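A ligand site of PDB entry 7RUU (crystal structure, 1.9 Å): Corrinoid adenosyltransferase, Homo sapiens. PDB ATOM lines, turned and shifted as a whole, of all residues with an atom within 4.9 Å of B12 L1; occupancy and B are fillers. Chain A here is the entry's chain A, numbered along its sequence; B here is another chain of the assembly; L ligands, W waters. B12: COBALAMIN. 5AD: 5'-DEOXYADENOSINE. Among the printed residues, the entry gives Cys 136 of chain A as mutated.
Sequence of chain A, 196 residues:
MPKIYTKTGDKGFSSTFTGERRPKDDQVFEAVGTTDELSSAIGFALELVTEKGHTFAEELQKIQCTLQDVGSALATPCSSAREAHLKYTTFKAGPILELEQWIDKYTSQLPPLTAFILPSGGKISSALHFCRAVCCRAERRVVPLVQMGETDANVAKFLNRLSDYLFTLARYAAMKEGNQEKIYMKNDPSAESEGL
Merely in contact with B12 L1: Leu 113 (3.3 Å), Ala 75 of chain B (3.4 Å), Phe 116 (3.4 Å), Ala 115 (3.5 Å), Phe 167 (3.5 Å), Asp 36 of chain B (3.7 Å) and Gly 71 of chain B (3.7 Å). Hydrophobic or aromatic side chains within 4 Å of B12 L1: Leu 113, Phe 116, Ile 117, Phe 167 and Ala 75 of chain B. 14 residues have an atom within 4 Å of B12 L1: Leu 113, Thr 114, Ala 115, Phe 116, Ile 117, Arg 132, Ser 163, Asp 164, Phe 167, Asp 36 of chain B, Gln 68 of chain B, Gly 71 of chain B, Ser 72 of chain B and Ala 75 of chain B. The nearest printed residue that does not touch B12 L1 is Val 32 of chain B (4.2 Å).
OG of Ser 72 of chain B lies within hydrogen-bond range of O of Gln 68 of chain B. NH2 of Arg 132 is in salt-bridge range of OD2 of Asp 36 of chain B, at 2.8 Å. The backbone carbonyl oxygen (O) of Arg 132 is in hydrogen-bond range of the side-chain sulfur (SG) of Cys 136.
The backbone carbonyl oxygen (O) of Thr 114 sits at hydrogen-bond distance from an oxygen (O7R) of B12 L1, 2.7 Å away. O44 of B12 L1 sits at hydrogen-bond distance from N of Ile 117, 3.0 Å away. O of Ile 117 lies within hydrogen-bond range of N45 of B12 L1, 2.8 Å away. An oxygen (O51) of B12 L1 lies within hydrogen-bond range of the backbone NH (N) of Ser 72 of chain B, at 3.3 Å. The side-chain hydroxyl (OG) of Ser 72 of chain B sits at hydrogen-bond distance from an oxygen (O51) of B12 L1 (2.9 Å). N40 of B12 L1 lies within hydrogen-bond range of OD1 of Asp 164, at 2.9 Å. The backbone carbonyl oxygen of Ser 163 lies within hydrogen-bond range of a nitrogen (N40) of B12 L1 (3.0 Å). O39 of B12 L1 is in hydrogen-bond range of NH2 of Arg 132. A nitrogen (N52) of B12 L1 sits at hydrogen-bond distance from the backbone carbonyl oxygen of Gln 68 of chain B, at 3.3 Å. O of Cys 136 is in hydrogen-bond range of N6 of 5AD L2, 2.9 Å away.
Water W8 lies within hydrogen-bond range of an oxygen (O5) of B12 L1 (2.6 Å) and the side-chain amide nitrogen (NE2) of Gln 68 of chain B (2.9 Å). Water W5 lies within hydrogen-bond range of O5 of B12 L1 and N of Phe 116. Water W4 lies within hydrogen-bond range of the side-chain carboxylate of Asp 36 of chain B (2.7 Å) and a nitrogen (N45) of B12 L1 (3.1 Å).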
ATOM      1  N   LEU A 113     -13.559  27.764  23.008  1.00  0.00           N
ATOM      2  CA  LEU A 113     -14.836  27.697  22.297  1.00  0.00           C
ATOM      3  C   LEU A 113     -15.928  27.652  23.350  1.00  0.00           C
ATOM      4  O   LEU A 113     -15.930  26.752  24.186  1.00  0.00           O
ATOM      5  CB  LEU A 113     -14.901  26.458  21.393  1.00  0.00           C
ATOM      6  CG  LEU A 113     -16.239  26.225  20.674  1.00  0.00           C
ATOM      7  CD1 LEU A 113     -16.537  27.391  19.744  1.00  0.00           C
ATOM      8  CD2 LEU A 113     -16.212  24.907  19.897  1.00  0.00           C
ATOM      9  N   THR A 114     -16.838  28.627  23.315  1.00  0.00           N
ATOM     10  CA  THR A 114     -17.974  28.645  24.227  1.00  0.00           C
ATOM     11  C   THR A 114     -19.288  28.783  23.456  1.00  0.00           C
ATOM     12  O   THR A 114     -20.257  29.387  23.943  1.00  0.00           O
ATOM     13  CB  THR A 114     -17.848  29.775  25.242  1.00  0.00           C
ATOM     14  OG1 THR A 114     -17.730  31.010  24.528  1.00  0.00           O
ATOM     15  CG2 THR A 114     -16.603  29.570  26.098  1.00  0.00           C
ATOM     16  N   ALA A 115     -19.347  28.210  22.254  1.00  0.00           N
ATOM     17  CA  ALA A 115     -20.496  28.392  21.391  1.00  0.00           C
ATOM     18  C   ALA A 115     -20.591  27.189  20.449  1.00  0.00           C
ATOM     19  O   ALA A 115     -19.593  26.522  20.179  1.00  0.00           O
ATOM     20  CB  ALA A 115     -20.383  29.694  20.585  1.00  0.00           C
ATOM     21  N   PHE A 116     -21.800  26.907  19.976  1.00  0.00           N
ATOM     22  CA  PHE A 116     -21.998  25.874  18.978  1.00  0.00           C
ATOM     23  C   PHE A 116     -21.284  26.268  17.689  1.00  0.00           C
ATOM     24  O   PHE A 116     -21.207  27.445  17.337  1.00  0.00           O
ATOM     25  CB  PHE A 116     -23.497  25.670  18.686  1.00  0.00           C
ATOM     26  CG  PHE A 116     -24.288  25.196  19.868  1.00  0.00           C
ATOM     27  CD1 PHE A 116     -24.068  23.935  20.381  1.00  0.00           C
ATOM     28  CD2 PHE A 116     -25.243  26.016  20.471  1.00  0.00           C
ATOM     29  CE1 PHE A 116     -24.781  23.471  21.484  1.00  0.00           C
ATOM     30  CE2 PHE A 116     -25.951  25.568  21.585  1.00  0.00           C
ATOM     31  CZ  PHE A 116     -25.722  24.288  22.086  1.00  0.00           C
ATOM     32  N   ILE A 117     -20.750  25.265  16.980  1.00  0.00           N
ATOM     33  CA  ILE A 117     -20.158  25.490  15.658  1.00  0.00           C
ATOM     34  C   ILE A 117     -21.052  24.853  14.608  1.00  0.00           C
ATOM     35  O   ILE A 117     -21.792  23.904  14.900  1.00  0.00           O
ATOM     36  CB  ILE A 117     -18.726  24.942  15.581  1.00  0.00           C
ATOM     37  CG1 ILE A 117     -18.701  23.443  15.868  1.00  0.00           C
ATOM     38  CG2 ILE A 117     -17.790  25.728  16.531  1.00  0.00           C
ATOM     39  CD1 ILE A 117     -17.303  22.803  15.828  1.00  0.00           C
ATOM     40  N   PRO A 119     -21.554  22.274  11.887  1.00  0.00           N
ATOM     41  CA  PRO A 119     -20.798  21.055  11.550  1.00  0.00           C
ATOM     42  C   PRO A 119     -20.246  21.168  10.138  1.00  0.00           C
ATOM     43  O   PRO A 119     -20.986  21.078   9.161  1.00  0.00           O
ATOM     44  CB  PRO A 119     -21.829  19.913  11.663  1.00  0.00           C
ATOM     45  CG  PRO A 119     -23.038  20.494  12.241  1.00  0.00           C
ATOM     46  CD  PRO A 119     -22.985  21.998  12.128  1.00  0.00           C
ATOM     47  N   ARG A 132     -20.135  11.649  14.984  1.00  0.00           N
ATOM     48  CA  ARG A 132     -20.495  12.137  16.311  1.00  0.00           C
ATOM     49  C   ARG A 132     -22.004  12.059  16.535  1.00  0.00           C
ATOM     50  O   ARG A 132     -22.472  11.596  17.593  1.00  0.00           O
ATOM     51  CB  ARG A 132     -19.968  13.571  16.463  1.00  0.00           C
ATOM     52  CG  ARG A 132     -20.292  14.306  17.800  1.00  0.00           C
ATOM     53  CD  ARG A 132     -19.964  15.826  17.716  1.00  0.00           C
ATOM     54  NE  ARG A 132     -20.624  16.445  16.546  1.00  0.00           N
ATOM     55  CZ  ARG A 132     -21.912  16.765  16.515  1.00  0.00           C
ATOM     56  NH1 ARG A 132     -22.447  17.272  15.417  1.00  0.00           N
ATOM     57  NH2 ARG A 132     -22.670  16.555  17.581  1.00  0.00           N
ATOM     58  N   CYS A 136     -24.110   9.680  19.200  1.00  0.00           N
ATOM     59  CA  CYS A 136     -25.161  10.086  20.138  1.00  0.00           C
ATOM     60  C   CYS A 136     -26.429   9.255  19.961  1.00  0.00           C
ATOM     61  O   CYS A 136     -27.102   8.903  20.946  1.00  0.00           O
ATOM     62  CB  CYS A 136     -25.452  11.568  19.978  1.00  0.00           C
ATOM     63  SG  CYS A 136     -24.132  12.594  20.707  1.00  0.00           S
ATOM     64  N   SER A 163     -18.518  10.491  21.818  1.00  0.00           N
ATOM     65  CA  SER A 163     -19.119  11.634  21.127  1.00  0.00           C
ATOM     66  C   SER A 163     -18.337  12.913  21.394  1.00  0.00           C
ATOM     67  O   SER A 163     -18.245  13.775  20.507  1.00  0.00           O
ATOM     68  CB  SER A 163     -20.592  11.792  21.517  1.00  0.00           C
ATOM     69  OG  SER A 163     -20.749  12.312  22.826  1.00  0.00           O
ATOM     70  N   ASP A 164     -17.753  13.054  22.590  1.00  0.00           N
ATOM     71  CA  ASP A 164     -16.885  14.205  22.863  1.00  0.00           C
ATOM     72  C   ASP A 164     -15.551  14.080  22.129  1.00  0.00           C
ATOM     73  O   ASP A 164     -15.006  15.084  21.641  1.00  0.00           O
ATOM     74  CB  ASP A 164     -16.638  14.340  24.375  1.00  0.00           C
ATOM     75  CG  ASP A 164     -17.879  14.833  25.122  1.00  0.00           C
ATOM     76  OD1 ASP A 164     -18.723  15.530  24.514  1.00  0.00           O
ATOM     77  OD2 ASP A 164     -17.992  14.541  26.332  1.00  0.00           O
ATOM     78  N   PHE A 167     -16.214  15.008  18.467  1.00  0.00           N
ATOM     79  CA  PHE A 167     -16.347  16.463  18.354  1.00  0.00           C
ATOM     80  C   PHE A 167     -14.979  17.142  18.385  1.00  0.00           C
ATOM     81  O   PHE A 167     -14.674  18.023  17.565  1.00  0.00           O
ATOM     82  CB  PHE A 167     -17.221  17.014  19.495  1.00  0.00           C
ATOM     83  CG  PHE A 167     -17.454  18.496  19.435  1.00  0.00           C
ATOM     84  CD1 PHE A 167     -18.355  19.036  18.523  1.00  0.00           C
ATOM     85  CD2 PHE A 167     -16.800  19.368  20.322  1.00  0.00           C
ATOM     86  CE1 PHE A 167     -18.585  20.409  18.457  1.00  0.00           C
ATOM     87  CE2 PHE A 167     -17.030  20.733  20.268  1.00  0.00           C
ATOM     88  CZ  PHE A 167     -17.920  21.262  19.349  1.00  0.00           C
ATOM     89  N   VAL B  32     -33.722  16.406  18.887  1.00  0.00           N
ATOM     90  CA  VAL B  32     -32.565  17.292  18.730  1.00  0.00           C
ATOM     91  C   VAL B  32     -31.377  16.520  18.181  1.00  0.00           C
ATOM     92  O   VAL B  32     -30.597  17.055  17.393  1.00  0.00           O
ATOM     93  CB  VAL B  32     -32.184  18.027  20.039  1.00  0.00           C
ATOM     94  CG1 VAL B  32     -33.259  19.052  20.419  1.00  0.00           C
ATOM     95  CG2 VAL B  32     -31.877  17.058  21.184  1.00  0.00           C
ATOM     96  N   GLY B  33     -31.240  15.251  18.560  1.00  0.00           N
ATOM     97  CA  GLY B  33     -30.174  14.427  18.008  1.00  0.00           C
ATOM     98  C   GLY B  33     -30.301  14.240  16.506  1.00  0.00           C
ATOM     99  O   GLY B  33     -29.303  14.322  15.788  1.00  0.00           O
ATOM    100  N   ASP B  36     -29.443  17.352  14.624  1.00  0.00           N
ATOM    101  CA  ASP B  36     -27.975  17.413  14.599  1.00  0.00           C
ATOM    102  C   ASP B  36     -27.398  16.475  13.534  1.00  0.00           C
ATOM    103  O   ASP B  36     -26.513  16.865  12.767  1.00  0.00           O
ATOM    104  CB  ASP B  36     -27.450  17.059  15.999  1.00  0.00           C
ATOM    105  CG  ASP B  36     -25.927  17.066  16.115  1.00  0.00           C
ATOM    106  OD1 ASP B  36     -25.214  17.751  15.337  1.00  0.00           O
ATOM    107  OD2 ASP B  36     -25.421  16.392  17.034  1.00  0.00           O
ATOM    108  N   LEU B  67     -31.050  25.241  11.405  1.00  0.00           N
ATOM    109  CA  LEU B  67     -31.137  23.978  12.146  1.00  0.00           C
ATOM    110  C   LEU B  67     -30.603  24.121  13.570  1.00  0.00           C
ATOM    111  O   LEU B  67     -31.081  23.437  14.483  1.00  0.00           O
ATOM    112  CB  LEU B  67     -30.400  22.851  11.405  1.00  0.00           C
ATOM    113  CG  LEU B  67     -31.067  22.422  10.081  1.00  0.00           C
ATOM    114  CD1 LEU B  67     -30.201  21.379   9.350  1.00  0.00           C
ATOM    115  CD2 LEU B  67     -32.463  21.832  10.307  1.00  0.00           C
ATOM    116  N   GLN B  68     -29.603  24.980  13.776  1.00  0.00           N
ATOM    117  CA  GLN B  68     -29.188  25.288  15.139  1.00  0.00           C
ATOM    118  C   GLN B  68     -30.336  25.949  15.916  1.00  0.00           C
ATOM    119  O   GLN B  68     -30.593  25.585  17.070  1.00  0.00           O
ATOM    120  CB  GLN B  68     -27.960  26.192  15.104  1.00  0.00           C
ATOM    121  CG  GLN B  68     -27.328  26.454  16.500  1.00  0.00           C
ATOM    122  CD  GLN B  68     -26.023  27.206  16.419  1.00  0.00           C
ATOM    123  OE1 GLN B  68     -25.138  26.841  15.666  1.00  0.00           O
ATOM    124  NE2 GLN B  68     -25.889  28.269  17.225  1.00  0.00           N
ATOM    125  N   GLY B  71     -32.820  23.334  16.857  1.00  0.00           N
ATOM    126  CA  GLY B  71     -32.389  22.580  18.023  1.00  0.00           C
ATOM    127  C   GLY B  71     -32.666  23.337  19.312  1.00  0.00           C
ATOM    128  O   GLY B  71     -33.152  22.761  20.289  1.00  0.00           O
ATOM    129  N   SER B  72     -32.390  24.648  19.311  1.00  0.00           N
ATOM    130  CA  SER B  72     -32.667  25.467  20.495  1.00  0.00           C
ATOM    131  C   SER B  72     -34.164  25.517  20.783  1.00  0.00           C
ATOM    132  O   SER B  72     -34.576  25.453  21.948  1.00  0.00           O
ATOM    133  CB  SER B  72     -32.114  26.887  20.321  1.00  0.00           C
ATOM    134  OG  SER B  72     -30.708  26.873  20.178  1.00  0.00           O
ATOM    135  N   ALA B  75     -35.348  22.275  22.372  1.00  0.00           N
ATOM    136  CA  ALA B  75     -34.788  22.000  23.683  1.00  0.00           C
ATOM    137  C   ALA B  75     -35.365  22.863  24.800  1.00  0.00           C
ATOM    138  O   ALA B  75     -35.195  22.517  25.973  1.00  0.00           O
ATOM    139  CB  ALA B  75     -33.275  22.192  23.668  1.00  0.00           C
HETATM  140 CO   B12 L   1     -25.144  20.553  23.676  1.00  0.00          CO
HETATM  141  N21 B12 L   1     -23.979  21.193  24.969  1.00  0.00           N
HETATM  142  N22 B12 L   1     -23.628  19.905  22.684  1.00  0.00           N
HETATM  143  N23 B12 L   1     -26.451  20.202  22.404  1.00  0.00           N
HETATM  144  N24 B12 L   1     -26.456  21.385  24.788  1.00  0.00           N
HETATM  145  C1  B12 L   1     -24.469  22.234  25.890  1.00  0.00           C
HETATM  146  C20 B12 L   1     -24.371  23.668  25.277  1.00  0.00           C
HETATM  147  C2  B12 L   1     -23.526  22.054  27.165  1.00  0.00           C
HETATM  148  C25 B12 L   1     -23.411  23.377  27.985  1.00  0.00           C
HETATM  149  C26 B12 L   1     -24.080  20.876  28.006  1.00  0.00           C
HETATM  150  C27 B12 L   1     -23.168  20.555  29.189  1.00  0.00           C
HETATM  151  O28 B12 L   1     -23.187  21.024  30.338  1.00  0.00           O
HETATM  152  N29 B12 L   1     -22.234  19.639  28.940  1.00  0.00           N
HETATM  153  C3  B12 L   1     -22.210  21.589  26.471  1.00  0.00           C
HETATM  154  C30 B12 L   1     -21.128  22.687  26.082  1.00  0.00           C
HETATM  155  C31 B12 L   1     -20.108  22.961  27.238  1.00  0.00           C
HETATM  156  C32 B12 L   1     -19.060  21.872  27.346  1.00  0.00           C
HETATM  157  O34 B12 L   1     -19.085  21.168  28.357  1.00  0.00           O
HETATM  158  N33 B12 L   1     -18.145  21.662  26.401  1.00  0.00           N
HETATM  159  C4  B12 L   1     -22.729  20.892  25.234  1.00  0.00           C
HETATM  160  C5  B12 L   1     -21.910  20.022  24.403  1.00  0.00           C
HETATM  161  C35 B12 L   1     -20.669  19.406  25.113  1.00  0.00           C
HETATM  162  C6  B12 L   1     -22.315  19.708  23.114  1.00  0.00           C
HETATM  163  C7  B12 L   1     -21.573  18.842  22.079  1.00  0.00           C
HETATM  164  C36 B12 L   1     -20.082  19.142  21.886  1.00  0.00           C
HETATM  165  C37 B12 L   1     -21.879  17.336  22.434  1.00  0.00           C
HETATM  166  C38 B12 L   1     -21.171  16.302  21.487  1.00  0.00           C
HETATM  167  O39 B12 L   1     -21.760  16.046  20.401  1.00  0.00           O
HETATM  168  N40 B12 L   1     -20.037  15.749  21.886  1.00  0.00           N
HETATM  169  C8  B12 L   1     -22.425  19.168  20.793  1.00  0.00           C
HETATM  170  C41 B12 L   1     -21.908  20.444  20.025  1.00  0.00           C
HETATM  171  C42 B12 L   1     -22.684  20.640  18.699  1.00  0.00           C
HETATM  172  C43 B12 L   1     -22.128  21.709  17.817  1.00  0.00           C
HETATM  173  O44 B12 L   1     -21.356  22.582  18.286  1.00  0.00           O
HETATM  174  N45 B12 L   1     -22.414  21.757  16.505  1.00  0.00           N
HETATM  175  C9  B12 L   1     -23.769  19.538  21.402  1.00  0.00           C
HETATM  176  C10 B12 L   1     -24.948  19.248  20.753  1.00  0.00           C
HETATM  177  C11 B12 L   1     -26.211  19.572  21.200  1.00  0.00           C
HETATM  178  C12 B12 L   1     -27.491  19.195  20.448  1.00  0.00           C
HETATM  179  C46 B12 L   1     -27.793  17.692  20.744  1.00  0.00           C
HETATM  180  C47 B12 L   1     -27.423  19.326  18.899  1.00  0.00           C
HETATM  181  C13 B12 L   1     -28.549  20.069  21.173  1.00  0.00           C
HETATM  182  C48 B12 L   1     -29.004  21.297  20.288  1.00  0.00           C
HETATM  183  C49 B12 L   1     -27.953  22.428  20.306  1.00  0.00           C
HETATM  184  C50 B12 L   1     -28.498  23.555  19.420  1.00  0.00           C
HETATM  185  O51 B12 L   1     -29.205  24.443  20.008  1.00  0.00           O
HETATM  186  N52 B12 L   1     -28.250  23.564  18.166  1.00  0.00           N
HETATM  187  C14 B12 L   1     -27.826  20.509  22.425  1.00  0.00           C
HETATM  188  C15 B12 L   1     -28.522  21.102  23.473  1.00  0.00           C
HETATM  189  C53 B12 L   1     -30.043  21.220  23.375  1.00  0.00           C
HETATM  190  C16 B12 L   1     -27.721  21.569  24.586  1.00  0.00           C
HETATM  191  C17 B12 L   1     -28.189  22.553  25.720  1.00  0.00           C
HETATM  192  C54 B12 L   1     -28.913  21.427  26.572  1.00  0.00           C
HETATM  193  C55 B12 L   1     -29.138  23.676  25.439  1.00  0.00           C
HETATM  194  C56 B12 L   1     -28.587  24.449  24.215  1.00  0.00           C
HETATM  195  C57 B12 L   1     -29.546  25.586  23.847  1.00  0.00           C
HETATM  196  O58 B12 L   1     -30.640  25.332  23.378  1.00  0.00           O
HETATM  197  N59 B12 L   1     -29.102  26.801  24.073  1.00  0.00           N
HETATM  198  C18 B12 L   1     -26.929  22.968  26.479  1.00  0.00           C
HETATM  199  C60 B12 L   1     -27.044  23.133  28.038  1.00  0.00           C
HETATM  200  C61 B12 L   1     -27.947  24.291  28.448  1.00  0.00           C
HETATM  201  O63 B12 L   1     -27.743  25.442  28.029  1.00  0.00           O
HETATM  202  N62 B12 L   1     -28.983  23.966  29.237  1.00  0.00           N
HETATM  203  C19 B12 L   1     -25.976  21.862  26.084  1.00  0.00           C
HETATM  204  C1P B12 L   1     -30.007  27.896  23.690  1.00  0.00           C
HETATM  205  C2P B12 L   1     -29.217  28.758  22.688  1.00  0.00           C
HETATM  206  C3P B12 L   1     -30.025  29.959  22.173  1.00  0.00           C
HETATM  207  O3  B12 L   1     -28.058  29.239  23.449  1.00  0.00           O
HETATM  208  O4  B12 L   1     -27.008  31.451  22.714  1.00  0.00           O
HETATM  209  O5  B12 L   1     -26.359  29.267  21.512  1.00  0.00           O
HETATM  210  P   B12 L   1     -26.786  30.009  22.792  1.00  0.00           P
HETATM  211  O2  B12 L   1     -25.638  29.724  23.903  1.00  0.00           O
HETATM  212  C3R B12 L   1     -25.181  28.430  24.157  1.00  0.00           C
HETATM  213  C2R B12 L   1     -23.737  28.196  23.815  1.00  0.00           C
HETATM  214  O7R B12 L   1     -22.930  29.282  24.166  1.00  0.00           O
HETATM  215  C1R B12 L   1     -23.435  26.965  24.710  1.00  0.00           C
HETATM  216  O6R B12 L   1     -24.100  27.267  25.922  1.00  0.00           O
HETATM  217  C4R B12 L   1     -25.095  28.301  25.713  1.00  0.00           C
HETATM  218  C5R B12 L   1     -26.412  28.003  26.433  1.00  0.00           C
HETATM  219  O8R B12 L   1     -27.030  26.787  25.889  1.00  0.00           O
HETATM  220  N1B B12 L   1     -22.036  26.715  25.076  1.00  0.00           N
HETATM  221  C8B B12 L   1     -21.139  25.879  24.413  1.00  0.00           C
HETATM  222  C2B B12 L   1     -21.379  27.244  26.123  1.00  0.00           C
HETATM  223  N3B B12 L   1     -20.128  26.815  26.197  1.00  0.00           N
HETATM  224  C9B B12 L   1     -19.953  25.933  25.124  1.00  0.00           C
HETATM  225  C4B B12 L   1     -18.838  25.187  24.690  1.00  0.00           C
HETATM  226  C5B B12 L   1     -19.011  24.394  23.541  1.00  0.00           C
HETATM  227  C5M B12 L   1     -17.867  23.548  23.024  1.00  0.00           C
HETATM  228  C6B B12 L   1     -20.266  24.334  22.811  1.00  0.00           C
HETATM  229  C6M B12 L   1     -20.401  23.472  21.584  1.00  0.00           C
HETATM  230  C7B B12 L   1     -21.366  25.106  23.255  1.00  0.00           C
HETATM  231  N1  5AD L   2     -28.537  12.236  21.926  1.00  0.00           N
HETATM  232  C2  5AD L   2     -29.106  13.470  21.852  1.00  0.00           C
HETATM  233  N3  5AD L   2     -29.029  14.583  22.610  1.00  0.00           N
HETATM  234  C4  5AD L   2     -28.177  14.300  23.642  1.00  0.00           C
HETATM  235  N9  5AD L   2     -27.813  15.190  24.686  1.00  0.00           N
HETATM  236  C8  5AD L   2     -26.921  14.430  25.471  1.00  0.00           C
HETATM  237  N7  5AD L   2     -26.691  13.186  25.074  1.00  0.00           N
HETATM  238  C5  5AD L   2     -27.505  13.115  23.906  1.00  0.00           C
HETATM  239  C6  5AD L   2     -27.709  12.055  23.000  1.00  0.00           C
HETATM  240  N6  5AD L   2     -27.106  10.860  23.130  1.00  0.00           N
HETATM  241  C1' 5AD L   2     -28.270  16.551  24.762  1.00  0.00           C
HETATM  242  C2' 5AD L   2     -28.355  17.073  26.268  1.00  0.00           C
HETATM  243  C3' 5AD L   2     -27.000  17.820  26.404  1.00  0.00           C
HETATM  244  C4' 5AD L   2     -26.819  18.345  24.966  1.00  0.00           C
HETATM  245  C5' 5AD L   2     -25.394  18.820  24.697  1.00  0.00           C
HETATM  246  O4' 5AD L   2     -27.194  17.283  24.129  1.00  0.00           O
HETATM  247  O2' 5AD L   2     -29.397  17.932  26.287  1.00  0.00           O
HETATM  248  O3' 5AD L   2     -27.073  18.802  27.350  1.00  0.00           O
HETATM  249  O   HOH W   1     -26.040  22.432  16.839  1.00  0.00           O
HETATM  250  O   HOH W   2     -18.114  26.820  28.046  1.00  0.00           O
HETATM  251  O   HOH W   3     -28.798  32.434  25.107  1.00  0.00           O
HETATM  252  O   HOH W   4     -25.060  20.470  15.460  1.00  0.00           O
HETATM  253  O   HOH W   5     -23.744  29.319  20.591  1.00  0.00           O
HETATM  254  O   HOH W   6     -22.709  17.430  27.226  1.00  0.00           O
HETATM  255  O   HOH W   7     -24.648  33.025  23.257  1.00  0.00           O
HETATM  256  O   HOH W   8     -27.497  29.658  19.174  1.00  0.00           O
